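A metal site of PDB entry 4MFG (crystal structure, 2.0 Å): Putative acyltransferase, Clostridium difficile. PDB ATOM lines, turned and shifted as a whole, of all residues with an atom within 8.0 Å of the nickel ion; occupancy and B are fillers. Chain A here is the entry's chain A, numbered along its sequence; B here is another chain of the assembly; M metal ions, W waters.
O of His 87 lies within hydrogen-bond range of N of Asp 105 (2.8 Å). The backbone NH of His 82 of chain B sits close to the side-chain amide oxygen of Gln 61 of chain B, 3.3 Å away. A ring nitrogen (ND1) of His 82 of chain B lies within hydrogen-bond range of the side-chain carboxylate (OD1) of Asp 62 of chain B, 2.8 Å away. The guanidinium group of Arg 46 is in hydrogen-bond range of a ring nitrogen (NE2) of His 67. A ring nitrogen (NE2) of His 67 lies within hydrogen-bond range of the side-chain carboxylate (OD1) of Asp 48 (3.0 Å). The backbone carbonyl oxygen (O) of His 67 sits at hydrogen-bond distance from the backbone NH (N) of Gly 88, at 3.1 Å. The backbone carbonyl oxygen (O) of Val 86 sits at hydrogen-bond distance from the backbone NH (N) of His 67.
Three residues have an atom within 4 Å of the nickel ion: His 67, His 87 and His 82 of chain B.
The nickel ion is bound by a ring nitrogen (NE2) of His 87 (2.1 Å), water W2 (2.1 Å), a ring nitrogen (NE2) of His 82 of chain B (2.1 Å), water W1 (2.1 Å) and a ring nitrogen (ND1) of His 67 (2.1 Å). The nickel ion has five donor atoms within binding distance.
Water W2 lies within hydrogen-bond range of the side-chain hydroxyl (OH) of Tyr 159 of chain B (2.8 Å) and the side-chain amide oxygen (OE1) of Gln 61 of chain B (2.9 Å).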
ATOM      1  N   ARG A  46      18.938 -17.526 -14.469  1.00  0.00           N
ATOM      2  CA  ARG A  46      17.517 -17.376 -14.175  1.00  0.00           C
ATOM      3  C   ARG A  46      17.120 -17.859 -12.798  1.00  0.00           C
ATOM      4  O   ARG A  46      17.039 -19.048 -12.553  1.00  0.00           O
ATOM      5  CB  ARG A  46      16.725 -18.125 -15.252  1.00  0.00           C
ATOM      6  CG  ARG A  46      15.236 -18.020 -15.120  1.00  0.00           C
ATOM      7  CD  ARG A  46      14.517 -18.266 -16.424  1.00  0.00           C
ATOM      8  NE  ARG A  46      14.674 -19.588 -17.012  1.00  0.00           N
ATOM      9  CZ  ARG A  46      13.797 -20.589 -16.872  1.00  0.00           C
ATOM     10  NH1 ARG A  46      14.022 -21.735 -17.492  1.00  0.00           N
ATOM     11  NH2 ARG A  46      12.719 -20.458 -16.119  1.00  0.00           N
ATOM     12  N   ASP A  48      14.217 -17.643 -11.144  1.00  0.00           N
ATOM     13  CA  ASP A  48      12.768 -17.569 -11.017  1.00  0.00           C
ATOM     14  C   ASP A  48      12.186 -18.759 -10.285  1.00  0.00           C
ATOM     15  O   ASP A  48      10.998 -18.815 -10.060  1.00  0.00           O
ATOM     16  CB  ASP A  48      12.098 -17.383 -12.388  1.00  0.00           C
ATOM     17  CG  ASP A  48      12.417 -18.502 -13.398  1.00  0.00           C
ATOM     18  OD1 ASP A  48      13.119 -19.501 -13.069  1.00  0.00           O
ATOM     19  OD2 ASP A  48      11.936 -18.403 -14.554  1.00  0.00           O
ATOM     20  N   GLU A  49      13.021 -19.745  -9.946  1.00  0.00           N
ATOM     21  CA  GLU A  49      12.586 -20.925  -9.193  1.00  0.00           C
ATOM     22  C   GLU A  49      13.460 -20.868  -7.957  1.00  0.00           C
ATOM     23  O   GLU A  49      13.186 -20.083  -7.081  1.00  0.00           O
ATOM     24  CB  GLU A  49      12.756 -22.204 -10.007  1.00  0.00           C
ATOM     25  CG  GLU A  49      12.155 -23.424  -9.339  1.00  0.00           C
ATOM     26  CD  GLU A  49      11.915 -24.589 -10.301  1.00  0.00           C
ATOM     27  OE1 GLU A  49      12.608 -24.717 -11.364  1.00  0.00           O
ATOM     28  OE2 GLU A  49      11.008 -25.395  -9.997  1.00  0.00           O
ATOM     29  N   GLY A  50      14.523 -21.627  -7.874  1.00  0.00           N
ATOM     30  CA  GLY A  50      15.413 -21.429  -6.762  1.00  0.00           C
ATOM     31  C   GLY A  50      16.158 -20.107  -7.008  1.00  0.00           C
ATOM     32  O   GLY A  50      16.508 -19.797  -8.159  1.00  0.00           O
ATOM     33  N   ILE A  65      24.243 -21.667 -18.269  1.00  0.00           N
ATOM     34  CA  ILE A  65      22.906 -21.555 -17.715  1.00  0.00           C
ATOM     35  C   ILE A  65      22.938 -21.854 -16.236  1.00  0.00           C
ATOM     36  O   ILE A  65      23.517 -22.865 -15.817  1.00  0.00           O
ATOM     37  CB  ILE A  65      21.983 -22.569 -18.358  1.00  0.00           C
ATOM     38  CG1 ILE A  65      21.816 -22.233 -19.808  1.00  0.00           C
ATOM     39  CG2 ILE A  65      20.600 -22.552 -17.720  1.00  0.00           C
ATOM     40  CD1 ILE A  65      21.378 -23.409 -20.604  1.00  0.00           C
ATOM     41  N   VAL A  66      22.351 -20.978 -15.457  1.00  0.00           N
ATOM     42  CA  VAL A  66      22.254 -21.148 -14.031  1.00  0.00           C
ATOM     43  C   VAL A  66      20.759 -21.036 -13.745  1.00  0.00           C
ATOM     44  O   VAL A  66      20.120 -20.060 -14.134  1.00  0.00           O
ATOM     45  CB  VAL A  66      23.065 -20.074 -13.282  1.00  0.00           C
ATOM     46  CG1 VAL A  66      23.120 -20.377 -11.803  1.00  0.00           C
ATOM     47  CG2 VAL A  66      24.462 -20.010 -13.857  1.00  0.00           C
ATOM     48  N   HIS A  67      20.215 -22.091 -13.148  1.00  0.00           N
ATOM     49  CA  HIS A  67      18.789 -22.226 -12.822  1.00  0.00           C
ATOM     50  C   HIS A  67      18.652 -23.332 -11.762  1.00  0.00           C
ATOM     51  O   HIS A  67      19.610 -24.074 -11.534  1.00  0.00           O
ATOM     52  CB  HIS A  67      18.034 -22.585 -14.100  1.00  0.00           C
ATOM     53  CG  HIS A  67      16.560 -22.587 -13.935  1.00  0.00           C
ATOM     54  ND1 HIS A  67      15.832 -23.755 -13.857  1.00  0.00           N
ATOM     55  CD2 HIS A  67      15.671 -21.585 -13.793  1.00  0.00           C
ATOM     56  CE1 HIS A  67      14.550 -23.458 -13.695  1.00  0.00           C
ATOM     57  NE2 HIS A  67      14.429 -22.148 -13.649  1.00  0.00           N
ATOM     58  N   GLY A  68      17.514 -23.486 -11.098  1.00  0.00           N
ATOM     59  CA  GLY A  68      17.462 -24.526 -10.118  1.00  0.00           C
ATOM     60  C   GLY A  68      16.145 -24.779  -9.444  1.00  0.00           C
ATOM     61  O   GLY A  68      15.368 -23.849  -9.251  1.00  0.00           O
ATOM     62  N   ASP A  69      15.885 -26.043  -9.122  1.00  0.00           N
ATOM     63  CA  ASP A  69      14.695 -26.396  -8.350  1.00  0.00           C
ATOM     64  C   ASP A  69      14.914 -25.769  -6.992  1.00  0.00           C
ATOM     65  O   ASP A  69      14.086 -25.038  -6.487  1.00  0.00           O
ATOM     66  CB  ASP A  69      14.517 -27.895  -8.206  1.00  0.00           C
ATOM     67  CG  ASP A  69      14.314 -28.598  -9.538  1.00  0.00           C
ATOM     68  OD1 ASP A  69      14.489 -27.965 -10.609  1.00  0.00           O
ATOM     69  OD2 ASP A  69      13.975 -29.790  -9.526  1.00  0.00           O
ATOM     70  N   ILE A  85      26.087 -26.036 -17.430  1.00  0.00           N
ATOM     71  CA  ILE A  85      24.813 -25.910 -16.749  1.00  0.00           C
ATOM     72  C   ILE A  85      25.033 -26.168 -15.268  1.00  0.00           C
ATOM     73  O   ILE A  85      25.413 -27.260 -14.872  1.00  0.00           O
ATOM     74  CB  ILE A  85      23.755 -26.915 -17.182  1.00  0.00           C
ATOM     75  CG1 ILE A  85      23.534 -26.880 -18.707  1.00  0.00           C
ATOM     76  CG2 ILE A  85      22.435 -26.594 -16.470  1.00  0.00           C
ATOM     77  CD1 ILE A  85      22.404 -27.795 -19.157  1.00  0.00           C
ATOM     78  N   VAL A  86      24.783 -25.141 -14.456  1.00  0.00           N
ATOM     79  CA  VAL A  86      24.935 -25.226 -13.010  1.00  0.00           C
ATOM     80  C   VAL A  86      23.529 -25.123 -12.440  1.00  0.00           C
ATOM     81  O   VAL A  86      22.927 -24.041 -12.423  1.00  0.00           O
ATOM     82  CB  VAL A  86      25.765 -24.069 -12.516  1.00  0.00           C
ATOM     83  CG1 VAL A  86      26.010 -24.201 -11.033  1.00  0.00           C
ATOM     84  CG2 VAL A  86      27.087 -24.004 -13.283  1.00  0.00           C
ATOM     85  N   HIS A  87      23.010 -26.235 -11.954  1.00  0.00           N
ATOM     86  CA  HIS A  87      21.615 -26.293 -11.616  1.00  0.00           C
ATOM     87  C   HIS A  87      21.228 -26.722 -10.201  1.00  0.00           C
ATOM     88  O   HIS A  87      21.143 -27.913  -9.904  1.00  0.00           O
ATOM     89  CB  HIS A  87      20.966 -27.208 -12.634  1.00  0.00           C
ATOM     90  CG  HIS A  87      19.495 -27.020 -12.756  1.00  0.00           C
ATOM     91  ND1 HIS A  87      18.586 -27.708 -11.975  1.00  0.00           N
ATOM     92  CD2 HIS A  87      18.769 -26.239 -13.589  1.00  0.00           C
ATOM     93  CE1 HIS A  87      17.365 -27.353 -12.311  1.00  0.00           C
ATOM     94  NE2 HIS A  87      17.450 -26.450 -13.282  1.00  0.00           N
ATOM     95  N   GLY A  88      20.956 -25.748  -9.346  1.00  0.00           N
ATOM     96  CA  GLY A  88      20.555 -26.005  -7.957  1.00  0.00           C
ATOM     97  C   GLY A  88      21.638 -26.595  -7.081  1.00  0.00           C
ATOM     98  O   GLY A  88      21.348 -27.173  -6.028  1.00  0.00           O
ATOM     99  N   ASP A 105      21.088 -30.572  -9.132  1.00  0.00           N
ATOM    100  CA  ASP A 105      20.628 -30.055  -7.849  1.00  0.00           C
ATOM    101  C   ASP A 105      21.164 -30.724  -6.631  1.00  0.00           C
ATOM    102  O   ASP A 105      21.261 -31.944  -6.563  1.00  0.00           O
ATOM    103  CB  ASP A 105      19.089 -30.053  -7.773  1.00  0.00           C
ATOM    104  CG  ASP A 105      18.453 -29.309  -8.931  1.00  0.00           C
ATOM    105  OD1 ASP A 105      18.502 -29.835 -10.068  1.00  0.00           O
ATOM    106  OD2 ASP A 105      17.867 -28.232  -8.698  1.00  0.00           O
ATOM    107  N   GLN B  61      12.983 -24.945 -22.987  1.00  0.00           N
ATOM    108  CA  GLN B  61      13.788 -24.157 -22.053  1.00  0.00           C
ATOM    109  C   GLN B  61      15.028 -23.480 -22.632  1.00  0.00           C
ATOM    110  O   GLN B  61      15.416 -23.671 -23.778  1.00  0.00           O
ATOM    111  CB  GLN B  61      14.113 -24.987 -20.810  1.00  0.00           C
ATOM    112  CG  GLN B  61      12.876 -25.434 -20.055  1.00  0.00           C
ATOM    113  CD  GLN B  61      13.202 -26.333 -18.890  1.00  0.00           C
ATOM    114  OE1 GLN B  61      14.278 -26.289 -18.307  1.00  0.00           O
ATOM    115  NE2 GLN B  61      12.244 -27.154 -18.528  1.00  0.00           N
ATOM    116  N   ASP B  62      15.627 -22.670 -21.784  1.00  0.00           N
ATOM    117  CA  ASP B  62      16.733 -21.779 -22.147  1.00  0.00           C
ATOM    118  C   ASP B  62      17.806 -22.444 -22.987  1.00  0.00           C
ATOM    119  O   ASP B  62      18.274 -23.514 -22.682  1.00  0.00           O
ATOM    120  CB  ASP B  62      17.367 -21.178 -20.907  1.00  0.00           C
ATOM    121  CG  ASP B  62      16.351 -20.918 -19.827  1.00  0.00           C
ATOM    122  OD1 ASP B  62      15.967 -21.883 -19.155  1.00  0.00           O
ATOM    123  OD2 ASP B  62      15.970 -19.772 -19.640  1.00  0.00           O
ATOM    124  N   GLY B  81      14.138 -29.782 -21.437  1.00  0.00           N
ATOM    125  CA  GLY B  81      15.122 -29.206 -20.516  1.00  0.00           C
ATOM    126  C   GLY B  81      16.184 -28.284 -21.079  1.00  0.00           C
ATOM    127  O   GLY B  81      16.529 -28.345 -22.251  1.00  0.00           O
ATOM    128  N   HIS B  82      16.731 -27.464 -20.199  1.00  0.00           N
ATOM    129  CA  HIS B  82      17.729 -26.476 -20.599  1.00  0.00           C
ATOM    130  C   HIS B  82      18.763 -27.002 -21.591  1.00  0.00           C
ATOM    131  O   HIS B  82      19.346 -28.051 -21.419  1.00  0.00           O
ATOM    132  CB  HIS B  82      18.531 -25.955 -19.390  1.00  0.00           C
ATOM    133  CG  HIS B  82      17.709 -25.506 -18.229  1.00  0.00           C
ATOM    134  ND1 HIS B  82      17.040 -24.304 -18.193  1.00  0.00           N
ATOM    135  CD2 HIS B  82      17.529 -26.068 -17.009  1.00  0.00           C
ATOM    136  CE1 HIS B  82      16.443 -24.179 -17.033  1.00  0.00           C
ATOM    137  NE2 HIS B  82      16.697 -25.243 -16.299  1.00  0.00           N
ATOM    138  N   MET B  99      17.759 -31.950 -19.089  1.00  0.00           N
ATOM    139  CA  MET B  99      18.604 -30.865 -19.554  1.00  0.00           C
ATOM    140  C   MET B  99      19.875 -31.415 -20.203  1.00  0.00           C
ATOM    141  O   MET B  99      20.479 -32.406 -19.779  1.00  0.00           O
ATOM    142  CB  MET B  99      18.896 -29.843 -18.430  1.00  0.00           C
ATOM    143  CG  MET B  99      19.723 -30.357 -17.292  1.00  0.00           C
ATOM    144  SD  MET B  99      19.948 -29.273 -15.860  1.00  0.00           S
ATOM    145  CE  MET B  99      18.387 -29.567 -15.042  1.00  0.00           C
ATOM    146  N   TRP B 158       4.310 -26.122 -13.842  1.00  0.00           N
ATOM    147  CA  TRP B 158       5.135 -25.062 -13.286  1.00  0.00           C
ATOM    148  C   TRP B 158       5.409 -24.064 -14.359  1.00  0.00           C
ATOM    149  O   TRP B 158       5.297 -22.855 -14.138  1.00  0.00           O
ATOM    150  CB  TRP B 158       6.468 -25.609 -12.760  1.00  0.00           C
ATOM    151  CG  TRP B 158       7.254 -24.577 -12.072  1.00  0.00           C
ATOM    152  CD1 TRP B 158       7.177 -24.239 -10.759  1.00  0.00           C
ATOM    153  CD2 TRP B 158       8.226 -23.710 -12.650  1.00  0.00           C
ATOM    154  NE1 TRP B 158       8.067 -23.224 -10.483  1.00  0.00           N
ATOM    155  CE2 TRP B 158       8.712 -22.880 -11.626  1.00  0.00           C
ATOM    156  CE3 TRP B 158       8.736 -23.570 -13.946  1.00  0.00           C
ATOM    157  CZ2 TRP B 158       9.696 -21.914 -11.846  1.00  0.00           C
ATOM    158  CZ3 TRP B 158       9.720 -22.606 -14.176  1.00  0.00           C
ATOM    159  CH2 TRP B 158      10.179 -21.780 -13.130  1.00  0.00           C
ATOM    160  N   TYR B 159       5.774 -24.568 -15.528  1.00  0.00           N
ATOM    161  CA  TYR B 159       6.084 -23.710 -16.664  1.00  0.00           C
ATOM    162  C   TYR B 159       4.910 -22.899 -17.205  1.00  0.00           C
ATOM    163  O   TYR B 159       5.098 -21.812 -17.700  1.00  0.00           O
ATOM    164  CB  TYR B 159       6.830 -24.474 -17.774  1.00  0.00           C
ATOM    165  CG  TYR B 159       8.338 -24.404 -17.556  1.00  0.00           C
ATOM    166  CD1 TYR B 159       9.061 -23.269 -17.944  1.00  0.00           C
ATOM    167  CD2 TYR B 159       9.034 -25.440 -16.922  1.00  0.00           C
ATOM    168  CE1 TYR B 159      10.409 -23.187 -17.721  1.00  0.00           C
ATOM    169  CE2 TYR B 159      10.388 -25.345 -16.702  1.00  0.00           C
ATOM    170  CZ  TYR B 159      11.059 -24.222 -17.116  1.00  0.00           C
ATOM    171  OH  TYR B 159      12.376 -24.137 -16.882  1.00  0.00           O
HETATM  172 NI    NI M   1      15.855 -25.776 -14.448  1.00  0.00          NI
HETATM  173  O   HOH W   1      15.184 -27.764 -14.593  1.00  0.00           O
HETATM  174  O   HOH W   2      14.006 -25.950 -15.416  1.00  0.00           O
